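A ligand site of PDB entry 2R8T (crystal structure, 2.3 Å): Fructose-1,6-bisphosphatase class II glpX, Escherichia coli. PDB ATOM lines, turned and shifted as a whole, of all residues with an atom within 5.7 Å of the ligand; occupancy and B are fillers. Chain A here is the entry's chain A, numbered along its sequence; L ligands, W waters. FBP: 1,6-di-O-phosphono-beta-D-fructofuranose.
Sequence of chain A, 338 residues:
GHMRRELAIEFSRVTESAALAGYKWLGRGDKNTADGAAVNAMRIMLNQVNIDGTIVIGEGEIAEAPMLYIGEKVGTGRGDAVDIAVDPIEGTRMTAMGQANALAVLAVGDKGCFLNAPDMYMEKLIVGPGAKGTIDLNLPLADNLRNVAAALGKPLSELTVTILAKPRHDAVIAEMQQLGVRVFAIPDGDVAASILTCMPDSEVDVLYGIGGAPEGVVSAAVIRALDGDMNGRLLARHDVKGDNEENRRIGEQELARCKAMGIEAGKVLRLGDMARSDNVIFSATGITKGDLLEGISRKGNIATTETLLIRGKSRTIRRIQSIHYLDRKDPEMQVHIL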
ATOM      1  N   LYS A  31      16.701 -15.598 -27.571  1.00  0.00           N
ATOM      2  CA  LYS A  31      17.555 -15.014 -26.540  1.00  0.00           C
ATOM      3  C   LYS A  31      18.906 -15.705 -26.470  1.00  0.00           C
ATOM      4  O   LYS A  31      19.974 -15.061 -26.482  1.00  0.00           O
ATOM      5  CB  LYS A  31      16.910 -15.217 -25.169  1.00  0.00           C
ATOM      6  CG  LYS A  31      16.166 -14.052 -24.589  1.00  0.00           C
ATOM      7  CD  LYS A  31      15.241 -14.506 -23.451  1.00  0.00           C
ATOM      8  CE  LYS A  31      15.697 -13.988 -22.075  1.00  0.00           C
ATOM      9  NZ  LYS A  31      14.495 -13.544 -21.251  1.00  0.00           N
ATOM     10  N   ASP A  87      29.995  -9.213 -20.328  1.00  0.00           N
ATOM     11  CA  ASP A  87      28.537  -9.278 -20.486  1.00  0.00           C
ATOM     12  C   ASP A  87      28.354  -9.143 -21.992  1.00  0.00           C
ATOM     13  O   ASP A  87      27.968  -8.081 -22.509  1.00  0.00           O
ATOM     14  CB  ASP A  87      27.847  -8.165 -19.685  1.00  0.00           C
ATOM     15  CG  ASP A  87      26.470  -8.558 -19.175  1.00  0.00           C
ATOM     16  OD1 ASP A  87      25.760  -9.386 -19.818  1.00  0.00           O
ATOM     17  OD2 ASP A  87      26.091  -8.062 -18.083  1.00  0.00           O
ATOM     18  N   ILE A  89      26.191  -9.814 -24.162  1.00  0.00           N
ATOM     19  CA  ILE A  89      25.027  -9.015 -24.496  1.00  0.00           C
ATOM     20  C   ILE A  89      24.334  -8.632 -23.220  1.00  0.00           C
ATOM     21  O   ILE A  89      23.846  -9.484 -22.472  1.00  0.00           O
ATOM     22  CB  ILE A  89      23.939  -9.727 -25.426  1.00  0.00           C
ATOM     23  CG1 ILE A  89      24.484 -10.085 -26.810  1.00  0.00           C
ATOM     24  CG2 ILE A  89      22.689  -8.819 -25.582  1.00  0.00           C
ATOM     25  CD1 ILE A  89      23.532 -10.922 -27.613  1.00  0.00           C
ATOM     26  N   GLU A  90      24.286  -7.353 -22.992  1.00  0.00           N
ATOM     27  CA  GLU A  90      23.427  -6.779 -21.993  1.00  0.00           C
ATOM     28  C   GLU A  90      22.153  -6.283 -22.728  1.00  0.00           C
ATOM     29  O   GLU A  90      22.224  -5.434 -23.617  1.00  0.00           O
ATOM     30  CB  GLU A  90      24.214  -5.682 -21.296  1.00  0.00           C
ATOM     31  CG  GLU A  90      23.482  -4.876 -20.393  1.00  0.00           C
ATOM     32  CD  GLU A  90      23.238  -5.461 -19.008  1.00  0.00           C
ATOM     33  OE1 GLU A  90      23.259  -6.702 -18.775  1.00  0.00           O
ATOM     34  OE2 GLU A  90      22.949  -4.610 -18.141  1.00  0.00           O
ATOM     35  N   GLY A  91      21.014  -6.892 -22.391  1.00  0.00           N
ATOM     36  CA  GLY A  91      19.805  -6.755 -23.185  1.00  0.00           C
ATOM     37  C   GLY A  91      19.587  -7.886 -24.192  1.00  0.00           C
ATOM     38  O   GLY A  91      19.291  -7.604 -25.360  1.00  0.00           O
ATOM     39  N   THR A  92      19.738  -9.140 -23.736  1.00  0.00           N
ATOM     40  CA  THR A  92      19.499 -10.319 -24.588  1.00  0.00           C
ATOM     41  C   THR A  92      18.035 -10.399 -25.098  1.00  0.00           C
ATOM     42  O   THR A  92      17.794 -10.651 -26.278  1.00  0.00           O
ATOM     43  CB  THR A  92      19.852 -11.652 -23.850  1.00  0.00           C
ATOM     44  OG1 THR A  92      21.173 -11.576 -23.296  1.00  0.00           O
ATOM     45  CG2 THR A  92      19.796 -12.793 -24.797  1.00  0.00           C
ATOM     46  N   ARG A  93      17.075 -10.169 -24.195  1.00  0.00           N
ATOM     47  CA  ARG A  93      15.639 -10.167 -24.545  1.00  0.00           C
ATOM     48  C   ARG A  93      15.336  -9.057 -25.551  1.00  0.00           C
ATOM     49  O   ARG A  93      14.604  -9.259 -26.550  1.00  0.00           O
ATOM     50  CB  ARG A  93      14.756 -10.026 -23.302  1.00  0.00           C
ATOM     51  CG  ARG A  93      13.262  -9.952 -23.669  1.00  0.00           C
ATOM     52  CD  ARG A  93      12.369  -9.425 -22.550  1.00  0.00           C
ATOM     53  NE  ARG A  93      12.799  -8.123 -22.020  1.00  0.00           N
ATOM     54  CZ  ARG A  93      12.540  -6.936 -22.588  1.00  0.00           C
ATOM     55  NH1 ARG A  93      11.879  -6.872 -23.747  1.00  0.00           N
ATOM     56  NH2 ARG A  93      12.965  -5.810 -21.988  1.00  0.00           N
ATOM     57  N   MET A  94      15.921  -7.891 -25.312  1.00  0.00           N
ATOM     58  CA  MET A  94      15.774  -6.792 -26.244  1.00  0.00           C
ATOM     59  C   MET A  94      16.350  -7.127 -27.600  1.00  0.00           C
ATOM     60  O   MET A  94      15.771  -6.740 -28.610  1.00  0.00           O
ATOM     61  CB  MET A  94      16.324  -5.503 -25.648  1.00  0.00           C
ATOM     62  CG  MET A  94      15.895  -5.378 -24.182  1.00  0.00           C
ATOM     63  SD  MET A  94      15.921  -3.719 -23.517  1.00  0.00           S
ATOM     64  CE  MET A  94      17.701  -3.498 -23.296  1.00  0.00           C
ATOM     65  N   TYR A 121      20.927 -10.919  -6.710  1.00  0.00           N
ATOM     66  CA  TYR A 121      20.499  -9.530  -6.777  1.00  0.00           C
ATOM     67  C   TYR A 121      21.320  -8.588  -5.895  1.00  0.00           C
ATOM     68  O   TYR A 121      21.853  -8.996  -4.865  1.00  0.00           O
ATOM     69  CB  TYR A 121      19.006  -9.437  -6.431  1.00  0.00           C
ATOM     70  CG  TYR A 121      18.105  -9.921  -7.571  1.00  0.00           C
ATOM     71  CD1 TYR A 121      17.329 -11.068  -7.427  1.00  0.00           C
ATOM     72  CD2 TYR A 121      18.050  -9.222  -8.805  1.00  0.00           C
ATOM     73  CE1 TYR A 121      16.491 -11.506  -8.473  1.00  0.00           C
ATOM     74  CE2 TYR A 121      17.242  -9.647  -9.838  1.00  0.00           C
ATOM     75  CZ  TYR A 121      16.461 -10.795  -9.681  1.00  0.00           C
ATOM     76  OH  TYR A 121      15.640 -11.238 -10.713  1.00  0.00           O
ATOM     77  N   LYS A 124      21.373  -1.062  -5.559  1.00  0.00           N
ATOM     78  CA  LYS A 124      22.380  -0.174  -6.102  1.00  0.00           C
ATOM     79  C   LYS A 124      21.951   1.250  -5.902  1.00  0.00           C
ATOM     80  O   LYS A 124      20.767   1.547  -5.995  1.00  0.00           O
ATOM     81  CB  LYS A 124      22.576  -0.398  -7.631  1.00  0.00           C
ATOM     82  CG  LYS A 124      23.123  -1.774  -8.010  1.00  0.00           C
ATOM     83  CD  LYS A 124      22.893  -2.158  -9.490  1.00  0.00           C
ATOM     84  CE  LYS A 124      23.194  -3.630  -9.703  1.00  0.00           C
ATOM     85  NZ  LYS A 124      23.176  -4.043 -11.165  1.00  0.00           N
ATOM     86  N   LEU A 164      15.093   0.053 -12.804  1.00  0.00           N
ATOM     87  CA  LEU A 164      14.439  -1.028 -13.563  1.00  0.00           C
ATOM     88  C   LEU A 164      12.923  -1.072 -13.318  1.00  0.00           C
ATOM     89  O   LEU A 164      12.451  -1.071 -12.163  1.00  0.00           O
ATOM     90  CB  LEU A 164      15.085  -2.400 -13.292  1.00  0.00           C
ATOM     91  CG  LEU A 164      16.539  -2.557 -13.687  1.00  0.00           C
ATOM     92  CD1 LEU A 164      17.091  -3.871 -13.130  1.00  0.00           C
ATOM     93  CD2 LEU A 164      16.722  -2.484 -15.255  1.00  0.00           C
ATOM     94  N   LYS A 166      10.362  -3.046 -12.844  1.00  0.00           N
ATOM     95  CA  LYS A 166      10.045  -4.403 -12.397  1.00  0.00           C
ATOM     96  C   LYS A 166       9.075  -4.376 -11.201  1.00  0.00           C
ATOM     97  O   LYS A 166       9.049  -3.411 -10.439  1.00  0.00           O
ATOM     98  CB  LYS A 166      11.321  -5.139 -12.009  1.00  0.00           C
ATOM     99  CG  LYS A 166      12.479  -5.026 -12.959  1.00  0.00           C
ATOM    100  CD  LYS A 166      12.495  -6.196 -13.956  1.00  0.00           C
ATOM    101  CE  LYS A 166      13.611  -6.006 -15.001  1.00  0.00           C
ATOM    102  NZ  LYS A 166      13.616  -7.114 -15.953  1.00  0.00           N
ATOM    103  N   ARG A 168       9.159  -5.748  -8.266  1.00  0.00           N
ATOM    104  CA  ARG A 168       9.880  -5.440  -7.022  1.00  0.00           C
ATOM    105  C   ARG A 168      10.043  -3.949  -6.732  1.00  0.00           C
ATOM    106  O   ARG A 168      10.333  -3.548  -5.585  1.00  0.00           O
ATOM    107  CB  ARG A 168      11.253  -6.121  -7.034  1.00  0.00           C
ATOM    108  CG  ARG A 168      12.198  -5.705  -8.196  1.00  0.00           C
ATOM    109  CD  ARG A 168      13.536  -6.423  -8.033  1.00  0.00           C
ATOM    110  NE  ARG A 168      14.545  -6.132  -9.036  1.00  0.00           N
ATOM    111  CZ  ARG A 168      14.652  -6.756 -10.215  1.00  0.00           C
ATOM    112  NH1 ARG A 168      15.618  -6.415 -11.064  1.00  0.00           N
ATOM    113  NH2 ARG A 168      13.788  -7.714 -10.584  1.00  0.00           N
ATOM    114  N   PRO A 187      13.080  -0.773 -19.044  1.00  0.00           N
ATOM    115  CA  PRO A 187      12.714  -2.170 -19.132  1.00  0.00           C
ATOM    116  C   PRO A 187      13.856  -3.089 -18.715  1.00  0.00           C
ATOM    117  O   PRO A 187      13.631  -4.041 -17.981  1.00  0.00           O
ATOM    118  CB  PRO A 187      12.368  -2.358 -20.620  1.00  0.00           C
ATOM    119  CG  PRO A 187      12.157  -1.002 -21.137  1.00  0.00           C
ATOM    120  CD  PRO A 187      13.130  -0.151 -20.371  1.00  0.00           C
ATOM    121  N   ASP A 188      15.072  -2.830 -19.165  1.00  0.00           N
ATOM    122  CA  ASP A 188      16.220  -3.679 -18.771  1.00  0.00           C
ATOM    123  C   ASP A 188      17.426  -2.819 -18.908  1.00  0.00           C
ATOM    124  O   ASP A 188      17.317  -1.748 -19.526  1.00  0.00           O
ATOM    125  CB  ASP A 188      16.393  -4.858 -19.733  1.00  0.00           C
ATOM    126  CG  ASP A 188      15.749  -6.160 -19.246  1.00  0.00           C
ATOM    127  OD1 ASP A 188      15.989  -6.585 -18.085  1.00  0.00           O
ATOM    128  OD2 ASP A 188      15.033  -6.785 -20.061  1.00  0.00           O
ATOM    129  N   GLY A 189      18.582  -3.284 -18.397  1.00  0.00           N
ATOM    130  CA  GLY A 189      19.886  -2.671 -18.732  1.00  0.00           C
ATOM    131  C   GLY A 189      20.432  -1.658 -17.745  1.00  0.00           C
ATOM    132  O   GLY A 189      20.603  -0.470 -18.099  1.00  0.00           O
ATOM    133  N   ASP A 190      20.726  -2.099 -16.519  1.00  0.00           N
ATOM    134  CA  ASP A 190      21.210  -1.124 -15.536  1.00  0.00           C
ATOM    135  C   ASP A 190      22.719  -0.868 -15.596  1.00  0.00           C
ATOM    136  O   ASP A 190      23.217   0.100 -15.008  1.00  0.00           O
ATOM    137  CB  ASP A 190      20.674  -1.369 -14.125  1.00  0.00           C
ATOM    138  CG  ASP A 190      21.164  -2.690 -13.471  1.00  0.00           C
ATOM    139  OD1 ASP A 190      21.818  -3.545 -14.126  1.00  0.00           O
ATOM    140  OD2 ASP A 190      20.825  -2.862 -12.277  1.00  0.00           O
ATOM    141  N   VAL A 191      23.435  -1.680 -16.384  1.00  0.00           N
ATOM    142  CA  VAL A 191      24.813  -1.326 -16.639  1.00  0.00           C
ATOM    143  C   VAL A 191      24.856  -0.046 -17.474  1.00  0.00           C
ATOM    144  O   VAL A 191      25.444   0.928 -17.033  1.00  0.00           O
ATOM    145  CB  VAL A 191      25.625  -2.459 -17.320  1.00  0.00           C
ATOM    146  CG1 VAL A 191      26.973  -1.961 -17.607  1.00  0.00           C
ATOM    147  CG2 VAL A 191      25.696  -3.711 -16.433  1.00  0.00           C
ATOM    148  N   ILE A 210      17.292  -2.537  -7.448  1.00  0.00           N
ATOM    149  CA  ILE A 210      17.854  -3.872  -7.373  1.00  0.00           C
ATOM    150  C   ILE A 210      17.958  -4.487  -8.787  1.00  0.00           C
ATOM    151  O   ILE A 210      16.959  -4.571  -9.531  1.00  0.00           O
ATOM    152  CB  ILE A 210      17.013  -4.777  -6.428  1.00  0.00           C
ATOM    153  CG1 ILE A 210      16.938  -4.195  -4.983  1.00  0.00           C
ATOM    154  CG2 ILE A 210      17.532  -6.215  -6.437  1.00  0.00           C
ATOM    155  CD1 ILE A 210      15.797  -4.768  -4.116  1.00  0.00           C
ATOM    156  N   GLY A 211      19.195  -4.878  -9.156  1.00  0.00           N
ATOM    157  CA  GLY A 211      19.477  -5.552 -10.432  1.00  0.00           C
ATOM    158  C   GLY A 211      20.516  -6.610 -10.175  1.00  0.00           C
ATOM    159  O   GLY A 211      20.732  -6.973  -9.004  1.00  0.00           O
ATOM    160  N   GLY A 212      21.171  -7.090 -11.238  1.00  0.00           N
ATOM    161  CA  GLY A 212      22.185  -8.152 -11.097  1.00  0.00           C
ATOM    162  C   GLY A 212      23.340  -7.694 -10.211  1.00  0.00           C
ATOM    163  O   GLY A 212      23.816  -6.560 -10.347  1.00  0.00           O
ATOM    164  N   GLU A 215      26.539  -7.336 -12.763  1.00  0.00           N
ATOM    165  CA  GLU A 215      26.304  -6.040 -13.406  1.00  0.00           C
ATOM    166  C   GLU A 215      26.696  -4.848 -12.496  1.00  0.00           C
ATOM    167  O   GLU A 215      27.346  -3.893 -12.957  1.00  0.00           O
ATOM    168  CB  GLU A 215      24.815  -5.942 -13.778  1.00  0.00           C
ATOM    169  CG  GLU A 215      24.408  -6.745 -15.017  1.00  0.00           C
ATOM    170  CD  GLU A 215      23.939  -8.168 -14.737  1.00  0.00           C
ATOM    171  OE1 GLU A 215      24.065  -8.703 -13.610  1.00  0.00           O
ATOM    172  OE2 GLU A 215      23.412  -8.789 -15.661  1.00  0.00           O
ATOM    173  N   LYS A 241      11.942 -11.350  -3.869  1.00  0.00           N
ATOM    174  CA  LYS A 241      10.784 -11.867  -4.570  1.00  0.00           C
ATOM    175  C   LYS A 241       9.870 -12.783  -3.730  1.00  0.00           C
ATOM    176  O   LYS A 241      10.290 -13.416  -2.741  1.00  0.00           O
ATOM    177  CB  LYS A 241      11.236 -12.558  -5.866  1.00  0.00           C
ATOM    178  CG  LYS A 241      12.069 -11.667  -6.777  1.00  0.00           C
ATOM    179  CD  LYS A 241      11.884 -12.049  -8.239  1.00  0.00           C
ATOM    180  CE  LYS A 241      12.610 -11.078  -9.155  1.00  0.00           C
ATOM    181  NZ  LYS A 241      12.389 -11.452 -10.570  1.00  0.00           N
HETATM  182  P1  FBP L   1      19.099  -9.367 -19.837  1.00  0.00           P
HETATM  183  O1P FBP L   1      19.108 -10.556 -18.863  1.00  0.00           O
HETATM  184  O2P FBP L   1      20.483  -9.378 -20.513  1.00  0.00           O
HETATM  185  O3P FBP L   1      17.956  -9.524 -20.828  1.00  0.00           O
HETATM  186  O1  FBP L   1      18.882  -8.026 -18.942  1.00  0.00           O
HETATM  187  C1  FBP L   1      19.966  -7.490 -18.245  1.00  0.00           C
HETATM  188  C2  FBP L   1      19.419  -6.861 -16.981  1.00  0.00           C
HETATM  189  O2  FBP L   1      18.340  -5.936 -17.276  1.00  0.00           O
HETATM  190  C3  FBP L   1      20.526  -6.140 -16.240  1.00  0.00           C
HETATM  191  O3  FBP L   1      20.712  -4.851 -16.771  1.00  0.00           O
HETATM  192  C4  FBP L   1      19.987  -6.154 -14.802  1.00  0.00           C
HETATM  193  O4  FBP L   1      21.006  -6.020 -13.828  1.00  0.00           O
HETATM  194  C5  FBP L   1      19.282  -7.501 -14.749  1.00  0.00           C
HETATM  195  O5  FBP L   1      18.964  -7.872 -16.095  1.00  0.00           O
HETATM  196  C6  FBP L   1      18.017  -7.449 -13.897  1.00  0.00           C
HETATM  197  O6  FBP L   1      17.512  -8.774 -13.798  1.00  0.00           O
HETATM  198  P2  FBP L   1      15.949  -9.206 -13.784  1.00  0.00           P
HETATM  199  O4P FBP L   1      15.369  -9.150 -15.202  1.00  0.00           O
HETATM  200  O5P FBP L   1      15.157  -8.270 -12.889  1.00  0.00           O
HETATM  201  O6P FBP L   1      15.882 -10.657 -13.340  1.00  0.00           O
HETATM  202  O   HOH W   1      16.771  -7.652 -21.997  1.00  0.00           O
HETATM  203  O   HOH W   2      21.349 -10.120 -17.669  1.00  0.00           O
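OD1 of Asp 188 lies within hydrogen-bond range of O2 of the ligand (2.6 Å). N of Asp 190 is in hydrogen-bond range of O3 of the ligand, 2.8 Å away. O4 of the ligand lies within hydrogen-bond range of OD1 of Asp 190, 2.6 Å away. OE2 of Glu 90 lies within hydrogen-bond range of O3 of the ligand (2.6 Å). An oxygen (O5P) of the ligand lies within salt-bridge range of the guanidinium group (NH1) of Arg 168, 2.6 Å away. OH of Tyr 121 is in hydrogen-bond range of O6P of the ligand, 2.7 Å away. The side-chain amino group (NZ) of Lys 166 is in salt-bridge range of an oxygen (O4P) of the ligand (2.8 Å). The backbone NH of Gly 212 is in hydrogen-bond range of an oxygen (O4) of the ligand (2.8 Å). N of Gly 189 lies within hydrogen-bond range of O2 of the ligand (2.9 Å). An oxygen (O2P) of the ligand is in hydrogen-bond range of the backbone NH (N) of Gly 91 (3.2 Å). N of Thr 92 lies within hydrogen-bond range of O2P of the ligand, at 3.3 Å.
The side-chain carboxylate of Asp 188 is in salt-bridge range of the side-chain amino group of Lys 166. The side-chain carboxylate (OD2) of Asp 188 lies within salt-bridge range of the guanidinium group (NH2) of Arg 93 (3.0 Å). The side-chain carboxylate (OD2) of Asp 190 is in salt-bridge range of the side-chain amino group (NZ) of Lys 124, at 2.9 Å. N of Val 191 sits close to OE2 of Glu 90, at 3.5 Å. NH1 of Arg 168 is in hydrogen-bond range of O of Ile 210 (2.7 Å). The side-chain hydroxyl (OH) of Tyr 121 sits at hydrogen-bond distance from the side-chain amino group (NZ) of Lys 241, 3.3 Å away. NZ of Lys 124 is in hydrogen-bond range of O of Gly 212, 2.7 Å away. OG1 of Thr 92 sits at hydrogen-bond distance from O of Ile 89.
O of Ile 89 touches O2P of the ligand, at 3.9 Å. N of Arg 93 touches O3P of the ligand (3.5 Å). NZ of Lys 124 touches O4 of the ligand, at 3.96 Å. CD1 of Leu 164 touches C6 of the ligand, 3.8 Å away. Gly 211 touches the ligand (C to O4, 3.7 Å). CG of Glu 215 touches O4 of the ligand, at 3.7 Å. 16 residues have an atom within 4 Å of the ligand: Ile 89, Glu 90, Gly 91, Thr 92, Arg 93, Tyr 121, Lys 124, Leu 164, Lys 166, Arg 168, Asp 188, Gly 189, Asp 190, Gly 211, Gly 212 and Glu 215. The nearest printed residue that does not touch the ligand is Val 191 (4.2 Å).
Water W1 lies within hydrogen-bond range of O3P of the ligand (2.5 Å), OD2 of Asp 188 (2.7 Å), N of Arg 93 (3.4 Å) and N of Met 94 (3.4 Å). Water W2 lies within hydrogen-bond range of O1P of the ligand (2.6 Å) and OE2 of Glu 215 (3.2 Å).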
